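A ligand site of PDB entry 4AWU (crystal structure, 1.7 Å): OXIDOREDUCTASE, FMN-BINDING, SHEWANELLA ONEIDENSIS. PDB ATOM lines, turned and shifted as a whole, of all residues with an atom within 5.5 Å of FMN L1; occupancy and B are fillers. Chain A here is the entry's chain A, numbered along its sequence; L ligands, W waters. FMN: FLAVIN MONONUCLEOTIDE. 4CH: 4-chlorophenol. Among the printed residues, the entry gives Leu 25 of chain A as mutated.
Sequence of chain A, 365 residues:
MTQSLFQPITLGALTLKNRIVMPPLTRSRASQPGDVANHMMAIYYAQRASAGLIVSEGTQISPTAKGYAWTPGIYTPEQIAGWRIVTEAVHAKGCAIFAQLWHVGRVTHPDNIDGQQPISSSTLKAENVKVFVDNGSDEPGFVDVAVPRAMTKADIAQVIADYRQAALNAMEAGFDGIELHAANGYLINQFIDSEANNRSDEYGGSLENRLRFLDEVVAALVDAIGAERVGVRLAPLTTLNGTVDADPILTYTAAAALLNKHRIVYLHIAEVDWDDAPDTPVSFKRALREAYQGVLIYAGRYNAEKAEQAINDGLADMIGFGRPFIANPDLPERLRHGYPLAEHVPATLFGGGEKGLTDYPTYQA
The side-chain amide oxygen (OE1) of Gln 100 lies close to the backbone NH (N) of Gly 58 (3.3 Å). The side-chain hydroxyl of Ser 56 lies within hydrogen-bond range of the backbone NH of Gln 100 (3.0 Å). OE2 of Glu 179 is in hydrogen-bond range of NE2 of Gln 100 (2.9 Å). A ring nitrogen (ND1) of His 181 lies within hydrogen-bond range of the backbone NH (N) of Ala 183 (3.3 Å). NE of Arg 27 is in hydrogen-bond range of O of Leu 349, at 2.8 Å. The backbone NH (N) of Ala 183 lies within hydrogen-bond range of the backbone carbonyl oxygen (O) of Arg 233. The backbone carbonyl oxygen of Trp 274 is in hydrogen-bond range of the guanidinium group of Arg 323, at 3.5 Å. The side-chain amide oxygen (OD1) of Asn 184 lies close to the side-chain carboxylate (OD2) of Asp 273, at 2.8 Å.
Pro 23 touches FMN L1 (CB to O2', 3.5 Å). CA of Leu 25 touches N5 of FMN L1 (3.4 Å). Asn 184 touches FMN L1. O of Val 272 touches C5' of FMN L1 (3.2 Å). CH2 of Trp 274 touches C8M of FMN L1, at 3.5 Å. Ala 299 touches FMN L1 (CB to O3', 3.9 Å). Gly 300 touches FMN L1. CA of Phe 321 touches O3P of FMN L1, 3.7 Å away. Pro 324 touches FMN L1 (CD to O3P, 3.8 Å). Leu 349 touches FMN L1 (CD2 to C7M, 3.9 Å). Phe 350 touches FMN L1 (CZ to C7M, 3.6 Å). Hydrophobic or aromatic side chains within 4 Å of FMN L1: Pro 23, Pro 24, Leu 25, His 181, Trp 274, Ala 299, Pro 324, Leu 349 and Phe 350. The nearest printed residue that does not touch FMN L1 is Glu 57 (4.1 Å).
The side-chain amide nitrogen of Gln 100 lies within hydrogen-bond range of an oxygen (O2) of FMN L1 (2.8 Å). N of Thr 26 is in hydrogen-bond range of N5 of FMN L1 (2.9 Å). The backbone NH (N) of Gly 58 sits at hydrogen-bond distance from an oxygen (O4) of FMN L1, 3.2 Å away. The backbone NH (N) of Arg 301 lies within hydrogen-bond range of an oxygen (O2P) of FMN L1 (2.8 Å). O2 of FMN L1 sits at hydrogen-bond distance from NE2 of His 181, 3.3 Å away. The side-chain amide nitrogen of Asn 184 sits at hydrogen-bond distance from an oxygen (O7) of 4CH L2. O of Pro 24 is in hydrogen-bond range of O2' of FMN L1. An oxygen (O3P) of FMN L1 sits at hydrogen-bond distance from the backbone NH of Gly 322, at 2.8 Å. An oxygen (O3') of FMN L1 lies within hydrogen-bond range of the guanidinium group of Arg 233, 2.6 Å away. O7 of 4CH L2 lies within hydrogen-bond range of NE2 of His 181 (2.8 Å). The backbone NH of Arg 323 sits at hydrogen-bond distance from an oxygen (O1P) of FMN L1 (2.8 Å). NH2 of Arg 323 lies within salt-bridge range of O2P of FMN L1 (2.8 Å). O4 of FMN L1 sits at hydrogen-bond distance from OG1 of Thr 26 (2.7 Å).
Water W1 lies within hydrogen-bond range of O3' of FMN L1 (2.6 Å), O of Val 272 (2.8 Å) and OD1 of Asp 273 (2.8 Å). Water W3 bridges an oxygen (O3P) of FMN L1 and the backbone carbonyl oxygen (O) of Tyr 302. Water W4 bridges the backbone NH of Trp 274 (2.7 Å) and an oxygen (O4') of FMN L1 (2.9 Å).
A nitrogen (N3) of FMN L1 sits close to an oxygen (O7) of 4CH L2 (3.4 Å).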
ATOM      1  N   PRO A  23      21.028  -6.301  -9.939  1.00  0.00           N
ATOM      2  CA  PRO A  23      21.320  -6.800 -11.285  1.00  0.00           C
ATOM      3  C   PRO A  23      21.114  -5.699 -12.311  1.00  0.00           C
ATOM      4  O   PRO A  23      20.562  -4.657 -11.981  1.00  0.00           O
ATOM      5  CB  PRO A  23      20.279  -7.894 -11.462  1.00  0.00           C
ATOM      6  CG  PRO A  23      19.100  -7.388 -10.708  1.00  0.00           C
ATOM      7  CD  PRO A  23      19.659  -6.642  -9.512  1.00  0.00           C
ATOM      8  N   PRO A  24      21.549  -5.940 -13.545  1.00  0.00           N
ATOM      9  CA  PRO A  24      21.408  -4.935 -14.599  1.00  0.00           C
ATOM     10  C   PRO A  24      19.949  -4.546 -14.783  1.00  0.00           C
ATOM     11  O   PRO A  24      19.097  -5.415 -14.935  1.00  0.00           O
ATOM     12  CB  PRO A  24      21.924  -5.645 -15.845  1.00  0.00           C
ATOM     13  CG  PRO A  24      22.734  -6.779 -15.353  1.00  0.00           C
ATOM     14  CD  PRO A  24      22.152  -7.188 -14.042  1.00  0.00           C
ATOM     15  N   LEU A  25      19.690  -3.239 -14.773  1.00  0.00           N
ATOM     16  CA  LEU A  25      18.345  -2.739 -14.980  1.00  0.00           C
ATOM     17  C   LEU A  25      18.370  -1.528 -15.907  1.00  0.00           C
ATOM     18  O   LEU A  25      18.657  -0.408 -15.484  1.00  0.00           O
ATOM     19  CB  LEU A  25      17.693  -2.359 -13.644  1.00  0.00           C
ATOM     20  CG  LEU A  25      17.524  -3.507 -12.651  1.00  0.00           C
ATOM     21  CD1 LEU A  25      17.417  -2.964 -11.240  1.00  0.00           C
ATOM     22  CD2 LEU A  25      16.313  -4.365 -13.002  1.00  0.00           C
ATOM     23  N   THR A  26      18.092  -1.776 -17.179  1.00  0.00           N
ATOM     24  CA  THR A  26      17.933  -0.740 -18.176  1.00  0.00           C
ATOM     25  C   THR A  26      16.883   0.266 -17.719  1.00  0.00           C
ATOM     26  O   THR A  26      15.752  -0.096 -17.433  1.00  0.00           O
ATOM     27  CB  THR A  26      17.518  -1.348 -19.529  1.00  0.00           C
ATOM     28  OG1 THR A  26      18.609  -2.117 -20.043  1.00  0.00           O
ATOM     29  CG2 THR A  26      17.138  -0.282 -20.535  1.00  0.00           C
ATOM     30  N   ARG A  27      17.287   1.536 -17.628  1.00  0.00           N
ATOM     31  CA  ARG A  27      16.381   2.610 -17.255  1.00  0.00           C
ATOM     32  C   ARG A  27      16.282   3.661 -18.357  1.00  0.00           C
ATOM     33  O   ARG A  27      15.442   4.558 -18.293  1.00  0.00           O
ATOM     34  CB  ARG A  27      16.837   3.254 -15.950  1.00  0.00           C
ATOM     35  CG  ARG A  27      17.107   2.268 -14.815  1.00  0.00           C
ATOM     36  CD  ARG A  27      15.901   1.371 -14.521  1.00  0.00           C
ATOM     37  NE  ARG A  27      14.696   2.160 -14.253  1.00  0.00           N
ATOM     38  CZ  ARG A  27      14.403   2.709 -13.081  1.00  0.00           C
ATOM     39  NH1 ARG A  27      15.213   2.559 -12.044  1.00  0.00           N
ATOM     40  NH2 ARG A  27      13.295   3.409 -12.939  1.00  0.00           N
ATOM     41  N   SER A  56      25.717  -2.703 -13.683  1.00  0.00           N
ATOM     42  CA  SER A  56      25.051  -1.621 -14.401  1.00  0.00           C
ATOM     43  C   SER A  56      24.036  -2.186 -15.367  1.00  0.00           C
ATOM     44  O   SER A  56      24.142  -3.340 -15.800  1.00  0.00           O
ATOM     45  CB  SER A  56      26.069  -0.798 -15.195  1.00  0.00           C
ATOM     46  OG  SER A  56      26.393  -1.431 -16.413  1.00  0.00           O
ATOM     47  N   GLU A  57      23.048  -1.377 -15.712  1.00  0.00           N
ATOM     48  CA  GLU A  57      22.212  -1.626 -16.869  1.00  0.00           C
ATOM     49  C   GLU A  57      23.084  -1.945 -18.076  1.00  0.00           C
ATOM     50  O   GLU A  57      24.244  -1.515 -18.155  1.00  0.00           O
ATOM     51  CB  GLU A  57      21.362  -0.397 -17.171  1.00  0.00           C
ATOM     52  CG  GLU A  57      22.168   0.836 -17.519  1.00  0.00           C
ATOM     53  CD  GLU A  57      21.472   2.113 -17.098  1.00  0.00           C
ATOM     54  OE1 GLU A  57      20.622   2.608 -17.866  1.00  0.00           O
ATOM     55  OE2 GLU A  57      21.781   2.629 -16.004  1.00  0.00           O
ATOM     56  N   GLY A  58      22.537  -2.701 -19.026  1.00  0.00           N
ATOM     57  CA  GLY A  58      23.249  -2.966 -20.266  1.00  0.00           C
ATOM     58  C   GLY A  58      23.786  -1.679 -20.845  1.00  0.00           C
ATOM     59  O   GLY A  58      23.082  -0.674 -20.906  1.00  0.00           O
ATOM     60  N   GLN A 100      27.739  -3.919 -17.388  1.00  0.00           N
ATOM     61  CA  GLN A 100      27.212  -4.968 -18.255  1.00  0.00           C
ATOM     62  C   GLN A 100      27.401  -4.585 -19.713  1.00  0.00           C
ATOM     63  O   GLN A 100      26.691  -3.720 -20.239  1.00  0.00           O
ATOM     64  CB  GLN A 100      25.728  -5.269 -18.007  1.00  0.00           C
ATOM     65  CG  GLN A 100      25.314  -6.519 -18.779  1.00  0.00           C
ATOM     66  CD  GLN A 100      23.833  -6.800 -18.758  1.00  0.00           C
ATOM     67  OE1 GLN A 100      23.025  -5.957 -19.155  1.00  0.00           O
ATOM     68  NE2 GLN A 100      23.458  -8.001 -18.334  1.00  0.00           N
ATOM     69  N   TRP A 102      27.008  -4.737 -23.488  1.00  0.00           N
ATOM     70  CA  TRP A 102      25.829  -5.116 -24.234  1.00  0.00           C
ATOM     71  C   TRP A 102      26.037  -5.056 -25.734  1.00  0.00           C
ATOM     72  O   TRP A 102      26.534  -4.056 -26.264  1.00  0.00           O
ATOM     73  CB  TRP A 102      24.709  -4.144 -23.883  1.00  0.00           C
ATOM     74  CG  TRP A 102      23.322  -4.664 -24.050  1.00  0.00           C
ATOM     75  CD1 TRP A 102      22.944  -5.927 -24.413  1.00  0.00           C
ATOM     76  CD2 TRP A 102      22.111  -3.925 -23.840  1.00  0.00           C
ATOM     77  NE1 TRP A 102      21.571  -6.017 -24.434  1.00  0.00           N
ATOM     78  CE2 TRP A 102      21.047  -4.806 -24.086  1.00  0.00           C
ATOM     79  CE3 TRP A 102      21.842  -2.616 -23.460  1.00  0.00           C
ATOM     80  CZ2 TRP A 102      19.712  -4.397 -23.974  1.00  0.00           C
ATOM     81  CZ3 TRP A 102      20.520  -2.219 -23.351  1.00  0.00           C
ATOM     82  CH2 TRP A 102      19.468  -3.111 -23.601  1.00  0.00           C
ATOM     83  N   GLU A 179      30.374  -7.332 -16.862  1.00  0.00           N
ATOM     84  CA  GLU A 179      29.520  -8.492 -17.035  1.00  0.00           C
ATOM     85  C   GLU A 179      29.168  -8.604 -18.504  1.00  0.00           C
ATOM     86  O   GLU A 179      28.609  -7.672 -19.087  1.00  0.00           O
ATOM     87  CB  GLU A 179      28.243  -8.369 -16.225  1.00  0.00           C
ATOM     88  CG  GLU A 179      27.353  -9.596 -16.323  1.00  0.00           C
ATOM     89  CD  GLU A 179      26.076  -9.442 -15.550  1.00  0.00           C
ATOM     90  OE1 GLU A 179      26.095  -9.713 -14.325  1.00  0.00           O
ATOM     91  OE2 GLU A 179      25.056  -9.063 -16.154  1.00  0.00           O
ATOM     92  N   HIS A 181      26.890  -9.522 -21.258  1.00  0.00           N
ATOM     93  CA  HIS A 181      25.483  -9.810 -21.436  1.00  0.00           C
ATOM     94  C   HIS A 181      25.329 -10.862 -22.521  1.00  0.00           C
ATOM     95  O   HIS A 181      25.339 -10.553 -23.708  1.00  0.00           O
ATOM     96  CB  HIS A 181      24.715  -8.548 -21.797  1.00  0.00           C
ATOM     97  CG  HIS A 181      23.232  -8.679 -21.625  1.00  0.00           C
ATOM     98  ND1 HIS A 181      22.618  -9.899 -21.435  1.00  0.00           N
ATOM     99  CD2 HIS A 181      22.247  -7.759 -21.609  1.00  0.00           C
ATOM    100  CE1 HIS A 181      21.321  -9.715 -21.302  1.00  0.00           C
ATOM    101  NE2 HIS A 181      21.065  -8.428 -21.404  1.00  0.00           N
ATOM    102  N   ALA A 183      22.678 -13.008 -22.527  1.00  0.00           N
ATOM    103  CA  ALA A 183      21.363 -13.474 -22.132  1.00  0.00           C
ATOM    104  C   ALA A 183      20.258 -12.756 -22.880  1.00  0.00           C
ATOM    105  O   ALA A 183      20.512 -11.916 -23.742  1.00  0.00           O
ATOM    106  CB  ALA A 183      21.180 -13.295 -20.618  1.00  0.00           C
ATOM    107  N   ASN A 184      19.020 -13.128 -22.549  1.00  0.00           N
ATOM    108  CA  ASN A 184      17.829 -12.452 -23.045  1.00  0.00           C
ATOM    109  C   ASN A 184      17.835 -12.184 -24.542  1.00  0.00           C
ATOM    110  O   ASN A 184      17.409 -11.113 -24.990  1.00  0.00           O
ATOM    111  CB  ASN A 184      17.580 -11.165 -22.252  1.00  0.00           C
ATOM    112  CG  ASN A 184      17.315 -11.430 -20.785  1.00  0.00           C
ATOM    113  OD1 ASN A 184      16.837 -12.502 -20.401  1.00  0.00           O
ATOM    114  ND2 ASN A 184      17.622 -10.452 -19.944  1.00  0.00           N
ATOM    115  N   ARG A 233      26.588 -13.185 -17.904  1.00  0.00           N
ATOM    116  CA  ARG A 233      25.194 -13.453 -17.585  1.00  0.00           C
ATOM    117  C   ARG A 233      24.549 -14.312 -18.664  1.00  0.00           C
ATOM    118  O   ARG A 233      24.639 -14.010 -19.852  1.00  0.00           O
ATOM    119  CB  ARG A 233      24.401 -12.169 -17.423  1.00  0.00           C
ATOM    120  CG  ARG A 233      23.074 -12.413 -16.725  1.00  0.00           C
ATOM    121  CD  ARG A 233      22.336 -11.143 -16.396  1.00  0.00           C
ATOM    122  NE  ARG A 233      21.517 -11.350 -15.202  1.00  0.00           N
ATOM    123  CZ  ARG A 233      20.423 -10.672 -14.902  1.00  0.00           C
ATOM    124  NH1 ARG A 233      19.969  -9.729 -15.714  1.00  0.00           N
ATOM    125  NH2 ARG A 233      19.776 -10.945 -13.782  1.00  0.00           N
ATOM    126  N   ALA A 270      20.052 -15.478 -15.050  1.00  0.00           N
ATOM    127  CA  ALA A 270      18.769 -14.793 -15.049  1.00  0.00           C
ATOM    128  C   ALA A 270      17.676 -15.831 -15.166  1.00  0.00           C
ATOM    129  O   ALA A 270      17.557 -16.505 -16.193  1.00  0.00           O
ATOM    130  CB  ALA A 270      18.702 -13.805 -16.198  1.00  0.00           C
ATOM    131  N   VAL A 272      14.232 -15.297 -14.337  1.00  0.00           N
ATOM    132  CA  VAL A 272      12.910 -14.790 -14.645  1.00  0.00           C
ATOM    133  C   VAL A 272      13.021 -13.495 -15.426  1.00  0.00           C
ATOM    134  O   VAL A 272      13.873 -12.656 -15.135  1.00  0.00           O
ATOM    135  CB  VAL A 272      12.113 -14.507 -13.373  1.00  0.00           C
ATOM    136  CG1 VAL A 272      10.773 -13.878 -13.732  1.00  0.00           C
ATOM    137  CG2 VAL A 272      11.927 -15.785 -12.578  1.00  0.00           C
ATOM    138  N   ASP A 273      12.146 -13.340 -16.408  1.00  0.00           N
ATOM    139  CA  ASP A 273      12.053 -12.088 -17.138  1.00  0.00           C
ATOM    140  C   ASP A 273      10.608 -11.649 -17.215  1.00  0.00           C
ATOM    141  O   ASP A 273       9.811 -12.223 -17.957  1.00  0.00           O
ATOM    142  CB  ASP A 273      12.666 -12.224 -18.531  1.00  0.00           C
ATOM    143  CG  ASP A 273      14.167 -12.155 -18.496  1.00  0.00           C
ATOM    144  OD1 ASP A 273      14.697 -11.027 -18.385  1.00  0.00           O
ATOM    145  OD2 ASP A 273      14.804 -13.225 -18.571  1.00  0.00           O
ATOM    146  N   TRP A 274      10.271 -10.645 -16.410  1.00  0.00           N
ATOM    147  CA  TRP A 274       8.914 -10.174 -16.290  1.00  0.00           C
ATOM    148  C   TRP A 274       8.036 -11.351 -15.824  1.00  0.00           C
ATOM    149  O   TRP A 274       8.241 -11.870 -14.725  1.00  0.00           O
ATOM    150  CB  TRP A 274       8.439  -9.572 -17.611  1.00  0.00           C
ATOM    151  CG  TRP A 274       9.431  -8.606 -18.232  1.00  0.00           C
ATOM    152  CD1 TRP A 274      10.312  -8.876 -19.242  1.00  0.00           C
ATOM    153  CD2 TRP A 274       9.649  -7.229 -17.872  1.00  0.00           C
ATOM    154  NE1 TRP A 274      11.057  -7.757 -19.538  1.00  0.00           N
ATOM    155  CE2 TRP A 274      10.667  -6.738 -18.718  1.00  0.00           C
ATOM    156  CE3 TRP A 274       9.081  -6.375 -16.924  1.00  0.00           C
ATOM    157  CZ2 TRP A 274      11.124  -5.423 -18.634  1.00  0.00           C
ATOM    158  CZ3 TRP A 274       9.534  -5.070 -16.854  1.00  0.00           C
ATOM    159  CH2 TRP A 274      10.541  -4.607 -17.705  1.00  0.00           C
ATOM    160  N   ALA A 299      19.166 -14.360 -10.268  1.00  0.00           N
ATOM    161  CA  ALA A 299      18.154 -13.327 -10.100  1.00  0.00           C
ATOM    162  C   ALA A 299      16.868 -13.797 -10.752  1.00  0.00           C
ATOM    163  O   ALA A 299      16.883 -14.472 -11.773  1.00  0.00           O
ATOM    164  CB  ALA A 299      18.601 -12.012 -10.720  1.00  0.00           C
ATOM    165  N   GLY A 300      15.743 -13.426 -10.156  1.00  0.00           N
ATOM    166  CA  GLY A 300      14.453 -13.796 -10.700  1.00  0.00           C
ATOM    167  C   GLY A 300      13.456 -14.148  -9.621  1.00  0.00           C
ATOM    168  O   GLY A 300      13.439 -15.260  -9.106  1.00  0.00           O
ATOM    169  N   ARG A 301      12.625 -13.161  -9.294  1.00  0.00           N
ATOM    170  CA  ARG A 301      11.557 -13.337  -8.308  1.00  0.00           C
ATOM    171  C   ARG A 301      12.069 -13.812  -6.951  1.00  0.00           C
ATOM    172  O   ARG A 301      11.377 -14.553  -6.255  1.00  0.00           O
ATOM    173  CB  ARG A 301      10.521 -14.331  -8.830  1.00  0.00           C
ATOM    174  CG  ARG A 301       9.650 -13.784  -9.943  1.00  0.00           C
ATOM    175  CD  ARG A 301       8.643 -14.831 -10.401  1.00  0.00           C
ATOM    176  NE  ARG A 301       7.670 -14.285 -11.331  1.00  0.00           N
ATOM    177  CZ  ARG A 301       6.625 -14.956 -11.805  1.00  0.00           C
ATOM    178  NH1 ARG A 301       6.413 -16.212 -11.436  1.00  0.00           N
ATOM    179  NH2 ARG A 301       5.778 -14.361 -12.645  1.00  0.00           N
ATOM    180  N   TYR A 302      13.267 -13.395  -6.562  1.00  0.00           N
ATOM    181  CA  TYR A 302      13.749 -13.767  -5.238  1.00  0.00           C
ATOM    182  C   TYR A 302      13.211 -12.794  -4.200  1.00  0.00           C
ATOM    183  O   TYR A 302      13.066 -11.597  -4.454  1.00  0.00           O
ATOM    184  CB  TYR A 302      15.269 -13.820  -5.174  1.00  0.00           C
ATOM    185  CG  TYR A 302      15.809 -15.083  -5.785  1.00  0.00           C
ATOM    186  CD1 TYR A 302      15.950 -16.228  -5.022  1.00  0.00           C
ATOM    187  CD2 TYR A 302      16.139 -15.143  -7.132  1.00  0.00           C
ATOM    188  CE1 TYR A 302      16.423 -17.405  -5.582  1.00  0.00           C
ATOM    189  CE2 TYR A 302      16.604 -16.309  -7.697  1.00  0.00           C
ATOM    190  CZ  TYR A 302      16.751 -17.436  -6.920  1.00  0.00           C
ATOM    191  OH  TYR A 302      17.211 -18.601  -7.477  1.00  0.00           O
ATOM    192  N   GLY A 320      20.478 -11.690  -6.945  1.00  0.00           N
ATOM    193  CA  GLY A 320      20.092 -10.392  -7.451  1.00  0.00           C
ATOM    194  C   GLY A 320      18.615 -10.131  -7.250  1.00  0.00           C
ATOM    195  O   GLY A 320      17.797 -11.043  -7.347  1.00  0.00           O
ATOM    196  N   PHE A 321      18.294  -8.878  -6.952  1.00  0.00           N
ATOM    197  CA  PHE A 321      16.922  -8.426  -6.828  1.00  0.00           C
ATOM    198  C   PHE A 321      16.782  -7.250  -7.776  1.00  0.00           C
ATOM    199  O   PHE A 321      17.373  -6.198  -7.559  1.00  0.00           O
ATOM    200  CB  PHE A 321      16.631  -7.977  -5.388  1.00  0.00           C
ATOM    201  CG  PHE A 321      16.881  -9.041  -4.352  1.00  0.00           C
ATOM    202  CD1 PHE A 321      18.160  -9.294  -3.885  1.00  0.00           C
ATOM    203  CD2 PHE A 321      15.836  -9.782  -3.828  1.00  0.00           C
ATOM    204  CE1 PHE A 321      18.384 -10.276  -2.935  1.00  0.00           C
ATOM    205  CE2 PHE A 321      16.053 -10.753  -2.883  1.00  0.00           C
ATOM    206  CZ  PHE A 321      17.328 -11.005  -2.430  1.00  0.00           C
ATOM    207  N   GLY A 322      16.021  -7.436  -8.849  1.00  0.00           N
ATOM    208  CA  GLY A 322      15.915  -6.414  -9.862  1.00  0.00           C
ATOM    209  C   GLY A 322      14.825  -5.414  -9.541  1.00  0.00           C
ATOM    210  O   GLY A 322      15.091  -4.313  -9.061  1.00  0.00           O
ATOM    211  N   ARG A 323      13.588  -5.808  -9.792  1.00  0.00           N
ATOM    212  CA  ARG A 323      12.466  -4.896  -9.633  1.00  0.00           C
ATOM    213  C   ARG A 323      12.371  -4.324  -8.216  1.00  0.00           C
ATOM    214  O   ARG A 323      12.087  -3.134  -8.055  1.00  0.00           O
ATOM    215  CB  ARG A 323      11.176  -5.576 -10.059  1.00  0.00           C
ATOM    216  CG  ARG A 323      11.031  -5.596 -11.578  1.00  0.00           C
ATOM    217  CD  ARG A 323      10.011  -6.601 -12.068  1.00  0.00           C
ATOM    218  NE  ARG A 323      10.513  -7.960 -11.986  1.00  0.00           N
ATOM    219  CZ  ARG A 323       9.858  -9.027 -12.420  1.00  0.00           C
ATOM    220  NH1 ARG A 323       8.657  -8.893 -12.964  1.00  0.00           N
ATOM    221  NH2 ARG A 323      10.394 -10.229 -12.293  1.00  0.00           N
ATOM    222  N   PRO A 324      12.611  -5.146  -7.186  1.00  0.00           N
ATOM    223  CA  PRO A 324      12.576  -4.539  -5.852  1.00  0.00           C
ATOM    224  C   PRO A 324      13.646  -3.469  -5.647  1.00  0.00           C
ATOM    225  O   PRO A 324      13.425  -2.545  -4.878  1.00  0.00           O
ATOM    226  CB  PRO A 324      12.792  -5.732  -4.920  1.00  0.00           C
ATOM    227  CG  PRO A 324      12.299  -6.904  -5.704  1.00  0.00           C
ATOM    228  CD  PRO A 324      12.700  -6.610  -7.121  1.00  0.00           C
ATOM    229  N   ILE A 326      14.569  -1.314  -7.817  1.00  0.00           N
ATOM    230  CA  ILE A 326      14.095  -0.119  -8.470  1.00  0.00           C
ATOM    231  C   ILE A 326      13.367   0.770  -7.475  1.00  0.00           C
ATOM    232  O   ILE A 326      13.638   1.961  -7.385  1.00  0.00           O
ATOM    233  CB  ILE A 326      13.153  -0.449  -9.635  1.00  0.00           C
ATOM    234  CG1 ILE A 326      13.927  -1.211 -10.714  1.00  0.00           C
ATOM    235  CG2 ILE A 326      12.531   0.840 -10.192  1.00  0.00           C
ATOM    236  CD1 ILE A 326      13.111  -1.573 -11.923  1.00  0.00           C
ATOM    237  N   LEU A 349       9.793   3.131 -15.599  1.00  0.00           N
ATOM    238  CA  LEU A 349      10.938   2.247 -15.735  1.00  0.00           C
ATOM    239  C   LEU A 349      11.938   2.810 -16.743  1.00  0.00           C
ATOM    240  O   LEU A 349      13.138   2.836 -16.483  1.00  0.00           O
ATOM    241  CB  LEU A 349      10.501   0.849 -16.158  1.00  0.00           C
ATOM    242  CG  LEU A 349       9.896  -0.050 -15.087  1.00  0.00           C
ATOM    243  CD1 LEU A 349       9.445  -1.376 -15.681  1.00  0.00           C
ATOM    244  CD2 LEU A 349      10.888  -0.286 -13.956  1.00  0.00           C
ATOM    245  N   PHE A 350      11.432   3.255 -17.890  1.00  0.00           N
ATOM    246  CA  PHE A 350      12.296   3.659 -18.989  1.00  0.00           C
ATOM    247  C   PHE A 350      12.036   5.097 -19.410  1.00  0.00           C
ATOM    248  O   PHE A 350      10.878   5.510 -19.554  1.00  0.00           O
ATOM    249  CB  PHE A 350      12.074   2.743 -20.197  1.00  0.00           C
ATOM    250  CG  PHE A 350      12.030   1.282 -19.852  1.00  0.00           C
ATOM    251  CD1 PHE A 350      13.192   0.608 -19.531  1.00  0.00           C
ATOM    252  CD2 PHE A 350      10.841   0.584 -19.867  1.00  0.00           C
ATOM    253  CE1 PHE A 350      13.165  -0.734 -19.217  1.00  0.00           C
ATOM    254  CE2 PHE A 350      10.805  -0.758 -19.557  1.00  0.00           C
ATOM    255  CZ  PHE A 350      11.964  -1.412 -19.228  1.00  0.00           C
HETATM  256  N1  FMN L   1      18.783  -7.820 -17.389  1.00  0.00           N
HETATM  257  C2  FMN L   1      19.972  -7.655 -18.056  1.00  0.00           C
HETATM  258  O2  FMN L   1      20.724  -8.614 -18.177  1.00  0.00           O
HETATM  259  N3  FMN L   1      20.309  -6.420 -18.594  1.00  0.00           N
HETATM  260  C4  FMN L   1      19.419  -5.368 -18.520  1.00  0.00           C
HETATM  261  O4  FMN L   1      19.788  -4.237 -18.842  1.00  0.00           O
HETATM  262  C4A FMN L   1      18.230  -5.534 -17.831  1.00  0.00           C
HETATM  263  N5  FMN L   1      17.345  -4.502 -17.730  1.00  0.00           N
HETATM  264  C5A FMN L   1      16.157  -4.668 -17.062  1.00  0.00           C
HETATM  265  C6  FMN L   1      15.307  -3.579 -16.911  1.00  0.00           C
HETATM  266  C7  FMN L   1      14.138  -3.697 -16.189  1.00  0.00           C
HETATM  267  C7M FMN L   1      13.249  -2.504 -16.053  1.00  0.00           C
HETATM  268  C8  FMN L   1      13.786  -4.940 -15.647  1.00  0.00           C
HETATM  269  C8M FMN L   1      12.539  -5.080 -14.830  1.00  0.00           C
HETATM  270  C9  FMN L   1      14.649  -6.020 -15.780  1.00  0.00           C
HETATM  271  C9A FMN L   1      15.850  -5.875 -16.451  1.00  0.00           C
HETATM  272  N10 FMN L   1      16.715  -6.945 -16.607  1.00  0.00           N
HETATM  273  C10 FMN L   1      17.900  -6.769 -17.288  1.00  0.00           C
HETATM  274  C1' FMN L   1      16.468  -8.248 -15.912  1.00  0.00           C
HETATM  275  C2' FMN L   1      16.800  -8.054 -14.436  1.00  0.00           C
HETATM  276  O2' FMN L   1      18.185  -7.824 -14.312  1.00  0.00           O
HETATM  277  C3' FMN L   1      16.410  -9.263 -13.573  1.00  0.00           C
HETATM  278  O3' FMN L   1      17.201 -10.367 -13.951  1.00  0.00           O
HETATM  279  C4' FMN L   1      14.915  -9.574 -13.719  1.00  0.00           C
HETATM  280  O4' FMN L   1      14.165  -8.393 -13.506  1.00  0.00           O
HETATM  281  C5' FMN L   1      14.439 -10.635 -12.740  1.00  0.00           C
HETATM  282  O5' FMN L   1      14.738 -10.278 -11.404  1.00  0.00           O
HETATM  283  P   FMN L   1      13.594  -9.684 -10.430  1.00  0.00           P
HETATM  284  O1P FMN L   1      13.191  -8.335 -10.960  1.00  0.00           O
HETATM  285  O2P FMN L   1      12.402 -10.613 -10.413  1.00  0.00           O
HETATM  286  O3P FMN L   1      14.174  -9.573  -9.041  1.00  0.00           O
HETATM  287 CL9  4CH L   2      14.477  -3.722 -20.333  1.00  0.00          CL
HETATM  288  C4  4CH L   2      15.581  -5.034 -20.460  1.00  0.00           C
HETATM  289  C5  4CH L   2      16.776  -4.838 -21.113  1.00  0.00           C
HETATM  290  C6  4CH L   2      17.691  -5.872 -21.209  1.00  0.00           C
HETATM  291  C1  4CH L   2      17.393  -7.110 -20.660  1.00  0.00           C
HETATM  292  O7  4CH L   2      18.311  -8.115 -20.755  1.00  0.00           O
HETATM  293  C2  4CH L   2      16.192  -7.315 -19.997  1.00  0.00           C
HETATM  294  C3  4CH L   2      15.278  -6.271 -19.902  1.00  0.00           C
HETATM  295  O   HOH W   1      16.232 -11.570 -16.071  1.00  0.00           O
HETATM  296  O   HOH W   2      10.493  -9.700  -8.322  1.00  0.00           O
HETATM  297  O   HOH W   3      12.779  -9.919  -6.730  1.00  0.00           O
HETATM  298  O   HOH W   4      12.112  -8.918 -15.549  1.00  0.00           O
HETATM  299  O   HOH W   5      15.320 -11.730  -7.890  1.00  0.00           O
